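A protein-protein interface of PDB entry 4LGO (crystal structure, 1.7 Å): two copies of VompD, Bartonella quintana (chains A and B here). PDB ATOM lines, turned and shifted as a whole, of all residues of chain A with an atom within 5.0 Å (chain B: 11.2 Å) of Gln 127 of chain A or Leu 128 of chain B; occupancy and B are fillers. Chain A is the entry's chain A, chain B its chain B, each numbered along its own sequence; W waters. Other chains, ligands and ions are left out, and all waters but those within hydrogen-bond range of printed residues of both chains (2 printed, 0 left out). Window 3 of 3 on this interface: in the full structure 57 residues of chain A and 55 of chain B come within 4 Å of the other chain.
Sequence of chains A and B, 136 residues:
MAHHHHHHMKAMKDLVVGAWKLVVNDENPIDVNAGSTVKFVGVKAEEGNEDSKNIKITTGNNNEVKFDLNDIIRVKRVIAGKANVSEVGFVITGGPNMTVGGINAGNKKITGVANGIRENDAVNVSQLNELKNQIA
The backbone NH (N) of Ala 114 of chain A lies within hydrogen-bond range of the backbone carbonyl oxygen (O) of Lys 108 of chain B (3.0 Å). The backbone NH of Ala 122 of chain A is in hydrogen-bond range of the backbone carbonyl oxygen of Ile 110 of chain B (2.9 Å). O of Val 123 of chain B is in hydrogen-bond range of N of Val 123 of chain A (3.3 Å).
The side-chain amide oxygen (OD1) of Asn 115 of chain A sits at hydrogen-bond distance from the side-chain amide nitrogen (ND2) of Asn 124 of chain A, 2.9 Å away. The backbone carbonyl oxygen of Ala 122 of chain A lies close to the backbone NH of Gly 116 of chain A (3.4 Å). O of Gly 116 of chain A lies within hydrogen-bond range of NE2 of Gln 127 of chain A (2.8 Å). OD1 of Asn 124 of chain A lies within hydrogen-bond range of N of Gln 127 of chain A (3.1 Å). The side-chain amide nitrogen (ND2) of Asn 124 of chain B lies within hydrogen-bond range of the backbone carbonyl oxygen (O) of Val 113 of chain B (2.9 Å). O of Val 125 of chain B lies close to ND2 of Asn 129 of chain B (3.5 Å).
Among the printed residues, merely in contact across the chains: Ala 114 of chain A with Lys 109 of chain B (3.7 Å), Asn 115 of chain A with Lys 109 of chain B (3.3 Å), Gly 116 of chain A with Val 125 of chain B (3.6 Å), Ala 122 of chain A with Val 113 of chain B (3.9 Å), Ala 122 of chain A with Val 123 of chain B (3.7 Å), Val 123 of chain A with Asn 124 of chain B (3.9 Å), Val 123 of chain A with Val 125 of chain B (3.6 Å), Val 123 of chain A with Leu 128 of chain B (3.8 Å), Gln 127 of chain A with Leu 128 of chain B (3.96 Å), Leu 131 of chain A with Leu 128 of chain B (3.5 Å) and Leu 131 of chain A with Lys 132 of chain B (3.6 Å).
Of the printed residues of chain B, Ala 114 of chain A touches Lys 108 and Lys 109. Of chain B, only Lys 109 (3.3 Å) comes within 4 Å of Asn 115 of chain A. Gly 116 of chain A touches just one residue of chain B: Val 125 (3.6 Å). Of the printed residues of chain B, Ala 122 of chain A touches Ile 110, Val 113 and Val 123. Val 123 of chain A touches just these residues of chain B: Val 123, Asn 124, Val 125 and Leu 128. No residue of chain B comes within 4 Å of Asn 124 of chain A. No residue of chain B comes within 4 Å of Val 125 of chain A. No residue of chain B comes within 4 Å of Ser 126 of chain A. Gln 127 of chain A touches one residue of chain B. No residue of chain B comes within 4 Å of Leu 128 of chain A. No residue of chain B comes within 4 Å of Asn 129 of chain A. No residue of chain B comes within 4 Å of Glu 130 of chain A. Leu 131 of chain A touches just these residues of chain B: Leu 128 (3.5 Å) and Lys 132 (3.6 Å). Printed residues of chain A within 4 Å of Asn 124 of chain B: Val 123. Leu 128 of chain B touches just these residues of chain A: Val 123 (3.8 Å), Gln 127 (3.96 Å) and Leu 131 (3.5 Å). The nearest residue of chain B that does not touch Gln 127 of chain A is Val 125 of chain B (4.9 Å). The nearest printed residue of chain A that does not touch Lys 108 of chain B is Asn 115 of chain A (5.9 Å).
Of the 13 printed residues of chain A, 7 touch a printed residue of chain B. Hydrophobic or aromatic side chains of chain A within 4 Å of the printed part of chain B: Ala 114, Ala 122, Val 123 and Leu 131. Hydrophobic or aromatic side chains of chain B within 4 Å of the printed part of chain A: Ile 110, Val 113, Val 123, Val 125 and Leu 128.
Ala 122 of chain A touches Val 123 of chain B, but with the chains exchanged Val 123 of chain A does not touch Ala 122 of chain B (6.6 Å). Val 123 of chain B touches its own counterpart, Val 123 of chain A. Val 123 of chain A touches Leu 128 of chain B, but with the chains exchanged Leu 128 of chain A does not touch Val 123 of chain B (7.0 Å). Leu 131 of chain A touches Leu 128 of chain B, but with the chains exchanged Leu 128 of chain A does not touch Leu 131 of chain B (5.7 Å). Positions printed for both chains: 114, 115, 116, 122, 123, 124, 125, 126, 127, 128, 129, 130 and 131. Of the 14 pairs that touch across the chains among the printed residues, 1 has its exchanged pair printed and touching as well.
Water W1 lies within hydrogen-bond range of O of Ala 122 of chain A, O of Ala 114 of chain A and N of Ile 110 of chain B. Water W2 lies within hydrogen-bond range of O of Val 123 of chain B and O of Val 123 of chain A.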
ATOM      1  N   ALA A 114      17.479 -30.001   6.103  1.00  0.00           N
ATOM      2  CA  ALA A 114      18.193 -30.647   7.190  1.00  0.00           C
ATOM      3  C   ALA A 114      19.699 -30.626   6.905  1.00  0.00           C
ATOM      4  O   ALA A 114      20.121 -30.538   5.749  1.00  0.00           O
ATOM      5  CB  ALA A 114      17.702 -32.084   7.389  1.00  0.00           C
ATOM      6  N   ASN A 115      20.503 -30.696   7.966  1.00  0.00           N
ATOM      7  CA  ASN A 115      21.950 -30.683   7.823  1.00  0.00           C
ATOM      8  C   ASN A 115      22.426 -31.704   6.813  1.00  0.00           C
ATOM      9  O   ASN A 115      22.062 -32.880   6.914  1.00  0.00           O
ATOM     10  CB  ASN A 115      22.645 -30.977   9.142  1.00  0.00           C
ATOM     11  CG  ASN A 115      22.641 -29.796  10.104  1.00  0.00           C
ATOM     12  OD1 ASN A 115      21.883 -28.836   9.972  1.00  0.00           O
ATOM     13  ND2 ASN A 115      23.498 -29.890  11.116  1.00  0.00           N
ATOM     14  N   GLY A 116      23.230 -31.255   5.849  1.00  0.00           N
ATOM     15  CA  GLY A 116      23.869 -32.165   4.900  1.00  0.00           C
ATOM     16  C   GLY A 116      24.916 -33.012   5.592  1.00  0.00           C
ATOM     17  O   GLY A 116      25.569 -32.536   6.544  1.00  0.00           O
ATOM     18  N   ALA A 122      23.253 -30.883   0.156  1.00  0.00           N
ATOM     19  CA  ALA A 122      23.226 -29.446   0.340  1.00  0.00           C
ATOM     20  C   ALA A 122      23.594 -29.108   1.777  1.00  0.00           C
ATOM     21  O   ALA A 122      23.368 -29.914   2.678  1.00  0.00           O
ATOM     22  CB  ALA A 122      21.839 -28.896   0.043  1.00  0.00           C
ATOM     23  N   VAL A 123      24.133 -27.910   1.977  1.00  0.00           N
ATOM     24  CA  VAL A 123      24.379 -27.398   3.333  1.00  0.00           C
ATOM     25  C   VAL A 123      23.419 -26.267   3.678  1.00  0.00           C
ATOM     26  O   VAL A 123      22.931 -25.534   2.807  1.00  0.00           O
ATOM     27  CB  VAL A 123      25.823 -26.927   3.538  1.00  0.00           C
ATOM     28  CG1 VAL A 123      26.776 -28.117   3.483  1.00  0.00           C
ATOM     29  CG2 VAL A 123      26.198 -25.895   2.529  1.00  0.00           C
ATOM     30  N   ASN A 124      23.161 -26.110   4.975  1.00  0.00           N
ATOM     31  CA  ASN A 124      22.343 -25.023   5.421  1.00  0.00           C
ATOM     32  C   ASN A 124      23.174 -23.951   6.157  1.00  0.00           C
ATOM     33  O   ASN A 124      24.396 -24.087   6.372  1.00  0.00           O
ATOM     34  CB  ASN A 124      21.138 -25.530   6.216  1.00  0.00           C
ATOM     35  CG  ASN A 124      21.528 -26.275   7.475  1.00  0.00           C
ATOM     36  OD1 ASN A 124      22.517 -25.942   8.134  1.00  0.00           O
ATOM     37  ND2 ASN A 124      20.726 -27.245   7.845  1.00  0.00           N
ATOM     38  N   VAL A 125      22.502 -22.853   6.444  1.00  0.00           N
ATOM     39  CA  VAL A 125      23.092 -21.724   7.121  1.00  0.00           C
ATOM     40  C   VAL A 125      23.686 -22.142   8.452  1.00  0.00           C
ATOM     41  O   VAL A 125      24.760 -21.657   8.808  1.00  0.00           O
ATOM     42  CB  VAL A 125      22.065 -20.603   7.310  1.00  0.00           C
ATOM     43  CG1 VAL A 125      22.583 -19.525   8.261  1.00  0.00           C
ATOM     44  CG2 VAL A 125      21.685 -20.015   5.942  1.00  0.00           C
ATOM     45  N   SER A 126      23.018 -23.037   9.181  1.00  0.00           N
ATOM     46  CA  SER A 126      23.593 -23.491  10.482  1.00  0.00           C
ATOM     47  C   SER A 126      24.989 -24.103  10.309  1.00  0.00           C
ATOM     48  O   SER A 126      25.882 -23.925  11.140  1.00  0.00           O
ATOM     49  CB  SER A 126      22.667 -24.472  11.215  1.00  0.00           C
ATOM     50  OG  SER A 126      22.808 -25.813  10.768  1.00  0.00           O
ATOM     51  N   GLN A 127      25.183 -24.795   9.191  1.00  0.00           N
ATOM     52  CA  GLN A 127      26.443 -25.419   8.907  1.00  0.00           C
ATOM     53  C   GLN A 127      27.481 -24.381   8.501  1.00  0.00           C
ATOM     54  O   GLN A 127      28.638 -24.517   8.880  1.00  0.00           O
ATOM     55  CB  GLN A 127      26.252 -26.511   7.829  1.00  0.00           C
ATOM     56  CG  GLN A 127      25.440 -27.680   8.357  1.00  0.00           C
ATOM     57  CD  GLN A 127      25.219 -28.758   7.319  1.00  0.00           C
ATOM     58  OE1 GLN A 127      24.472 -28.565   6.354  1.00  0.00           O
ATOM     59  NE2 GLN A 127      25.827 -29.915   7.548  1.00  0.00           N
ATOM     60  N   LEU A 128      27.073 -23.369   7.725  1.00  0.00           N
ATOM     61  CA  LEU A 128      27.954 -22.245   7.356  1.00  0.00           C
ATOM     62  C   LEU A 128      28.381 -21.506   8.620  1.00  0.00           C
ATOM     63  O   LEU A 128      29.559 -21.204   8.790  1.00  0.00           O
ATOM     64  CB  LEU A 128      27.287 -21.305   6.351  1.00  0.00           C
ATOM     65  CG  LEU A 128      28.080 -20.073   5.915  1.00  0.00           C
ATOM     66  CD1 LEU A 128      29.404 -20.486   5.293  1.00  0.00           C
ATOM     67  CD2 LEU A 128      27.286 -19.180   4.978  1.00  0.00           C
ATOM     68  N   ASN A 129      27.436 -21.303   9.545  1.00  0.00           N
ATOM     69  CA  ASN A 129      27.757 -20.707  10.852  1.00  0.00           C
ATOM     70  C   ASN A 129      28.699 -21.581  11.707  1.00  0.00           C
ATOM     71  O   ASN A 129      29.583 -21.033  12.392  1.00  0.00           O
ATOM     72  CB  ASN A 129      26.485 -20.359  11.647  1.00  0.00           C
ATOM     73  CG  ASN A 129      25.692 -19.227  11.014  1.00  0.00           C
ATOM     74  OD1 ASN A 129      26.220 -18.451  10.211  1.00  0.00           O
ATOM     75  ND2 ASN A 129      24.428 -19.107  11.395  1.00  0.00           N
ATOM     76  N   GLU A 130      28.534 -22.907  11.669  1.00  0.00           N
ATOM     77  CA  GLU A 130      29.488 -23.806  12.349  1.00  0.00           C
ATOM     78  C   GLU A 130      30.900 -23.594  11.826  1.00  0.00           C
ATOM     79  O   GLU A 130      31.829 -23.534  12.591  1.00  0.00           O
ATOM     80  CB  GLU A 130      29.169 -25.287  12.128  1.00  0.00           C
ATOM     81  CG  GLU A 130      28.065 -25.900  12.943  1.00  0.00           C
ATOM     82  CD  GLU A 130      28.035 -27.422  12.733  1.00  0.00           C
ATOM     83  OE1 GLU A 130      28.808 -28.126  13.425  1.00  0.00           O
ATOM     84  OE2 GLU A 130      27.278 -27.910  11.860  1.00  0.00           O
ATOM     85  N   LEU A 131      31.051 -23.518  10.503  1.00  0.00           N
ATOM     86  CA  LEU A 131      32.357 -23.248   9.888  1.00  0.00           C
ATOM     87  C   LEU A 131      32.943 -21.902  10.326  1.00  0.00           C
ATOM     88  O   LEU A 131      34.124 -21.802  10.704  1.00  0.00           O
ATOM     89  CB  LEU A 131      32.224 -23.294   8.365  1.00  0.00           C
ATOM     90  CG  LEU A 131      33.525 -23.100   7.584  1.00  0.00           C
ATOM     91  CD1 LEU A 131      34.554 -24.141   7.973  1.00  0.00           C
ATOM     92  CD2 LEU A 131      33.263 -23.210   6.090  1.00  0.00           C
ATOM     93  N   ALA B 105      12.188 -28.037   1.717  1.00  0.00           N
ATOM     94  CA  ALA B 105      12.800 -29.365   1.659  1.00  0.00           C
ATOM     95  C   ALA B 105      12.222 -30.338   2.701  1.00  0.00           C
ATOM     96  O   ALA B 105      12.695 -31.467   2.865  1.00  0.00           O
ATOM     97  CB  ALA B 105      14.312 -29.223   1.799  1.00  0.00           C
ATOM     98  N   LYS B 108      14.195 -32.353   5.655  1.00  0.00           N
ATOM     99  CA  LYS B 108      14.923 -33.525   5.187  1.00  0.00           C
ATOM    100  C   LYS B 108      16.155 -33.006   4.444  1.00  0.00           C
ATOM    101  O   LYS B 108      16.232 -31.817   4.087  1.00  0.00           O
ATOM    102  CB  LYS B 108      14.048 -34.347   4.211  1.00  0.00           C
ATOM    103  CG  LYS B 108      12.706 -34.819   4.751  1.00  0.00           C
ATOM    104  CD  LYS B 108      12.885 -35.993   5.681  1.00  0.00           C
ATOM    105  CE  LYS B 108      11.535 -36.602   6.061  1.00  0.00           C
ATOM    106  NZ  LYS B 108      11.784 -37.630   7.090  1.00  0.00           N
ATOM    107  N   LYS B 109      17.121 -33.884   4.215  1.00  0.00           N
ATOM    108  CA  LYS B 109      18.317 -33.508   3.471  1.00  0.00           C
ATOM    109  C   LYS B 109      17.991 -33.310   2.003  1.00  0.00           C
ATOM    110  O   LYS B 109      17.006 -33.860   1.496  1.00  0.00           O
ATOM    111  CB  LYS B 109      19.412 -34.559   3.626  1.00  0.00           C
ATOM    112  CG  LYS B 109      19.877 -34.714   5.061  1.00  0.00           C
ATOM    113  CD  LYS B 109      21.118 -35.580   5.195  1.00  0.00           C
ATOM    114  CE  LYS B 109      20.839 -37.028   4.824  1.00  0.00           C
ATOM    115  NZ  LYS B 109      19.800 -37.659   5.682  1.00  0.00           N
ATOM    116  N   ILE B 110      18.794 -32.493   1.336  1.00  0.00           N
ATOM    117  CA  ILE B 110      18.782 -32.431  -0.116  1.00  0.00           C
ATOM    118  C   ILE B 110      20.030 -33.155  -0.572  1.00  0.00           C
ATOM    119  O   ILE B 110      21.141 -32.770  -0.206  1.00  0.00           O
ATOM    120  CB  ILE B 110      18.772 -31.000  -0.693  1.00  0.00           C
ATOM    121  CG1 ILE B 110      17.544 -30.230  -0.162  1.00  0.00           C
ATOM    122  CG2 ILE B 110      18.833 -31.090  -2.219  1.00  0.00           C
ATOM    123  CD1 ILE B 110      17.446 -28.800  -0.636  1.00  0.00           C
ATOM    124  N   THR B 111      19.860 -34.202  -1.373  1.00  0.00           N
ATOM    125  CA  THR B 111      21.003 -34.986  -1.804  1.00  0.00           C
ATOM    126  C   THR B 111      21.230 -34.896  -3.303  1.00  0.00           C
ATOM    127  O   THR B 111      20.446 -34.308  -4.024  1.00  0.00           O
ATOM    128  CB  THR B 111      20.856 -36.445  -1.436  1.00  0.00           C
ATOM    129  OG1 THR B 111      22.190 -37.051  -1.535  1.00  0.00           O
ATOM    130  CG2 THR B 111      19.786 -37.061  -2.323  1.00  0.00           C
ATOM    131  N   VAL B 113      23.513 -33.288  -5.032  1.00  0.00           N
ATOM    132  CA  VAL B 113      23.828 -31.927  -5.438  1.00  0.00           C
ATOM    133  C   VAL B 113      25.240 -31.805  -6.013  1.00  0.00           C
ATOM    134  O   VAL B 113      26.238 -31.990  -5.317  1.00  0.00           O
ATOM    135  CB  VAL B 113      23.699 -30.974  -4.223  1.00  0.00           C
ATOM    136  CG1 VAL B 113      23.985 -29.520  -4.641  1.00  0.00           C
ATOM    137  CG2 VAL B 113      22.335 -31.104  -3.582  1.00  0.00           C
ATOM    138  N   ALA B 114      25.341 -31.484  -7.298  1.00  0.00           N
ATOM    139  CA  ALA B 114      26.627 -31.228  -7.921  1.00  0.00           C
ATOM    140  C   ALA B 114      27.195 -29.901  -7.417  1.00  0.00           C
ATOM    141  O   ALA B 114      26.433 -28.996  -7.060  1.00  0.00           O
ATOM    142  CB  ALA B 114      26.453 -31.166  -9.433  1.00  0.00           C
ATOM    143  N   ASN B 115      28.515 -29.788  -7.372  1.00  0.00           N
ATOM    144  CA  ASN B 115      29.163 -28.577  -6.877  1.00  0.00           C
ATOM    145  C   ASN B 115      28.624 -27.330  -7.564  1.00  0.00           C
ATOM    146  O   ASN B 115      28.592 -27.264  -8.782  1.00  0.00           O
ATOM    147  CB  ASN B 115      30.674 -28.620  -7.141  1.00  0.00           C
ATOM    148  CG  ASN B 115      31.420 -29.565  -6.212  1.00  0.00           C
ATOM    149  OD1 ASN B 115      30.843 -30.450  -5.582  1.00  0.00           O
ATOM    150  ND2 ASN B 115      32.727 -29.350  -6.112  1.00  0.00           N
ATOM    151  N   GLY B 116      28.217 -26.351  -6.778  1.00  0.00           N
ATOM    152  CA  GLY B 116      27.820 -25.052  -7.330  1.00  0.00           C
ATOM    153  C   GLY B 116      28.959 -24.295  -7.961  1.00  0.00           C
ATOM    154  O   GLY B 116      30.111 -24.387  -7.504  1.00  0.00           O
ATOM    155  N   ASP B 121      24.172 -20.585  -7.277  1.00  0.00           N
ATOM    156  CA  ASP B 121      24.098 -22.040  -7.203  1.00  0.00           C
ATOM    157  C   ASP B 121      24.192 -22.485  -5.738  1.00  0.00           C
ATOM    158  O   ASP B 121      24.917 -21.881  -4.926  1.00  0.00           O
ATOM    159  CB  ASP B 121      25.223 -22.724  -7.998  1.00  0.00           C
ATOM    160  CG  ASP B 121      25.134 -22.507  -9.525  1.00  0.00           C
ATOM    161  OD1 ASP B 121      24.105 -22.037 -10.054  1.00  0.00           O
ATOM    162  OD2 ASP B 121      26.115 -22.854 -10.212  1.00  0.00           O
ATOM    163  N   ALA B 122      23.494 -23.569  -5.399  1.00  0.00           N
ATOM    164  CA  ALA B 122      23.664 -24.161  -4.076  1.00  0.00           C
ATOM    165  C   ALA B 122      25.066 -24.744  -3.908  1.00  0.00           C
ATOM    166  O   ALA B 122      25.667 -25.202  -4.863  1.00  0.00           O
ATOM    167  CB  ALA B 122      22.616 -25.231  -3.833  1.00  0.00           C
ATOM    168  N   VAL B 123      25.573 -24.746  -2.673  1.00  0.00           N
ATOM    169  CA  VAL B 123      26.799 -25.450  -2.373  1.00  0.00           C
ATOM    170  C   VAL B 123      26.503 -26.716  -1.580  1.00  0.00           C
ATOM    171  O   VAL B 123      25.504 -26.824  -0.843  1.00  0.00           O
ATOM    172  CB  VAL B 123      27.827 -24.609  -1.609  1.00  0.00           C
ATOM    173  CG1 VAL B 123      28.260 -23.400  -2.421  1.00  0.00           C
ATOM    174  CG2 VAL B 123      27.285 -24.193  -0.268  1.00  0.00           C
ATOM    175  N   ASN B 124      27.406 -27.673  -1.726  1.00  0.00           N
ATOM    176  CA  ASN B 124      27.293 -28.932  -1.023  1.00  0.00           C
ATOM    177  C   ASN B 124      28.357 -29.077   0.068  1.00  0.00           C
ATOM    178  O   ASN B 124      29.239 -28.213   0.233  1.00  0.00           O
ATOM    179  CB  ASN B 124      27.291 -30.101  -2.002  1.00  0.00           C
ATOM    180  CG  ASN B 124      28.595 -30.234  -2.800  1.00  0.00           C
ATOM    181  OD1 ASN B 124      29.693 -29.899  -2.330  1.00  0.00           O
ATOM    182  ND2 ASN B 124      28.468 -30.716  -4.024  1.00  0.00           N
ATOM    183  N   VAL B 125      28.230 -30.169   0.814  1.00  0.00           N
ATOM    184  CA  VAL B 125      29.147 -30.510   1.914  1.00  0.00           C
ATOM    185  C   VAL B 125      30.604 -30.532   1.451  1.00  0.00           C
ATOM    186  O   VAL B 125      31.489 -29.996   2.167  1.00  0.00           O
ATOM    187  CB  VAL B 125      28.750 -31.852   2.566  1.00  0.00           C
ATOM    188  CG1 VAL B 125      29.820 -32.365   3.513  1.00  0.00           C
ATOM    189  CG2 VAL B 125      27.438 -31.692   3.315  1.00  0.00           C
ATOM    190  N   SER B 126      30.886 -31.132   0.291  1.00  0.00           N
ATOM    191  CA  SER B 126      32.274 -31.170  -0.206  1.00  0.00           C
ATOM    192  C   SER B 126      32.865 -29.766  -0.352  1.00  0.00           C
ATOM    193  O   SER B 126      34.047 -29.556  -0.062  1.00  0.00           O
ATOM    194  CB  SER B 126      32.442 -31.932  -1.536  1.00  0.00           C
ATOM    195  OG  SER B 126      32.017 -31.188  -2.657  1.00  0.00           O
ATOM    196  N   GLN B 127      32.047 -28.818  -0.797  1.00  0.00           N
ATOM    197  CA  GLN B 127      32.516 -27.427  -0.975  1.00  0.00           C
ATOM    198  C   GLN B 127      32.765 -26.731   0.364  1.00  0.00           C
ATOM    199  O   GLN B 127      33.730 -25.988   0.530  1.00  0.00           O
ATOM    200  CB  GLN B 127      31.542 -26.658  -1.831  1.00  0.00           C
ATOM    201  CG  GLN B 127      31.478 -27.222  -3.239  1.00  0.00           C
ATOM    202  CD  GLN B 127      30.531 -26.461  -4.134  1.00  0.00           C
ATOM    203  OE1 GLN B 127      29.314 -26.563  -3.997  1.00  0.00           O
ATOM    204  NE2 GLN B 127      31.091 -25.690  -5.072  1.00  0.00           N
ATOM    205  N   LEU B 128      31.908 -26.989   1.340  1.00  0.00           N
ATOM    206  CA  LEU B 128      32.136 -26.454   2.676  1.00  0.00           C
ATOM    207  C   LEU B 128      33.451 -27.015   3.259  1.00  0.00           C
ATOM    208  O   LEU B 128      34.281 -26.280   3.826  1.00  0.00           O
ATOM    209  CB  LEU B 128      30.925 -26.793   3.542  1.00  0.00           C
ATOM    210  CG  LEU B 128      30.707 -25.974   4.802  1.00  0.00           C
ATOM    211  CD1 LEU B 128      30.521 -24.512   4.415  1.00  0.00           C
ATOM    212  CD2 LEU B 128      29.477 -26.465   5.533  1.00  0.00           C
ATOM    213  N   ASN B 129      33.635 -28.320   3.110  1.00  0.00           N
ATOM    214  CA  ASN B 129      34.866 -29.000   3.532  1.00  0.00           C
ATOM    215  C   ASN B 129      36.131 -28.492   2.828  1.00  0.00           C
ATOM    216  O   ASN B 129      37.204 -28.410   3.448  1.00  0.00           O
ATOM    217  CB  ASN B 129      34.735 -30.519   3.320  1.00  0.00           C
ATOM    218  CG  ASN B 129      33.845 -31.185   4.363  1.00  0.00           C
ATOM    219  OD1 ASN B 129      33.676 -30.676   5.471  1.00  0.00           O
ATOM    220  ND2 ASN B 129      33.300 -32.329   4.024  1.00  0.00           N
ATOM    221  N   GLU B 130      36.022 -28.145   1.549  1.00  0.00           N
ATOM    222  CA  GLU B 130      37.187 -27.595   0.841  1.00  0.00           C
ATOM    223  C   GLU B 130      37.625 -26.300   1.534  1.00  0.00           C
ATOM    224  O   GLU B 130      38.809 -26.094   1.811  1.00  0.00           O
ATOM    225  CB  GLU B 130      36.878 -27.331  -0.636  1.00  0.00           C
ATOM    226  N   LEU B 131      36.654 -25.437   1.823  1.00  0.00           N
ATOM    227  CA  LEU B 131      36.932 -24.145   2.429  1.00  0.00           C
ATOM    228  C   LEU B 131      37.523 -24.362   3.816  1.00  0.00           C
ATOM    229  O   LEU B 131      38.515 -23.738   4.195  1.00  0.00           O
ATOM    230  CB  LEU B 131      35.659 -23.295   2.500  1.00  0.00           C
ATOM    231  CG  LEU B 131      35.819 -21.909   3.142  1.00  0.00           C
ATOM    232  CD1 LEU B 131      37.067 -21.215   2.624  1.00  0.00           C
ATOM    233  CD2 LEU B 131      34.581 -21.055   2.913  1.00  0.00           C
ATOM    234  N   LYS B 132      36.934 -25.306   4.544  1.00  0.00           N
ATOM    235  CA  LYS B 132      37.383 -25.685   5.878  1.00  0.00           C
ATOM    236  C   LYS B 132      38.842 -26.138   5.936  1.00  0.00           C
ATOM    237  O   LYS B 132      39.495 -26.030   6.986  1.00  0.00           O
ATOM    238  CB  LYS B 132      36.470 -26.792   6.379  1.00  0.00           C
ATOM    239  CG  LYS B 132      36.661 -27.222   7.815  1.00  0.00           C
ATOM    240  CD  LYS B 132      35.946 -28.542   8.073  1.00  0.00           C
ATOM    241  CE  LYS B 132      34.466 -28.523   7.706  1.00  0.00           C
ATOM    242  NZ  LYS B 132      33.611 -27.846   8.719  1.00  0.00           N
ATOM    243  N   ASN B 133      39.369 -26.645   4.826  1.00  0.00           N
ATOM    244  CA  ASN B 133      40.783 -27.028   4.785  1.00  0.00           C
ATOM    245  C   ASN B 133      41.695 -25.928   4.213  1.00  0.00           C
ATOM    246  O   ASN B 133      42.914 -25.976   4.389  1.00  0.00           O
ATOM    247  CB  ASN B 133      40.947 -28.385   4.096  1.00  0.00           C
ATOM    248  CG  ASN B 133      40.480 -29.528   4.987  1.00  0.00           C
ATOM    249  OD1 ASN B 133      41.165 -29.895   5.940  1.00  0.00           O
ATOM    250  ND2 ASN B 133      39.299 -30.057   4.719  1.00  0.00           N
ATOM    251  N   GLN B 134      41.104 -24.923   3.574  1.00  0.00           N
ATOM    252  CA  GLN B 134      41.802 -23.675   3.274  1.00  0.00           C
ATOM    253  C   GLN B 134      41.210 -22.537   4.119  1.00  0.00           C
ATOM    254  O   GLN B 134      41.839 -21.504   4.342  1.00  0.00           O
ATOM    255  CB  GLN B 134      41.716 -23.370   1.773  1.00  0.00           C
ATOM    256  CG  GLN B 134      40.386 -22.800   1.307  1.00  0.00           C
ATOM    257  CD  GLN B 134      40.088 -23.071  -0.162  1.00  0.00           C
ATOM    258  OE1 GLN B 134      40.614 -24.013  -0.755  1.00  0.00           O
ATOM    259  NE2 GLN B 134      39.221 -22.254  -0.751  1.00  0.00           N
HETATM  260  O   HOH W   1      20.925 -31.396   3.098  1.00  0.00           O
HETATM  261  O   HOH W   2      23.065 -25.443  -0.120  1.00  0.00           O
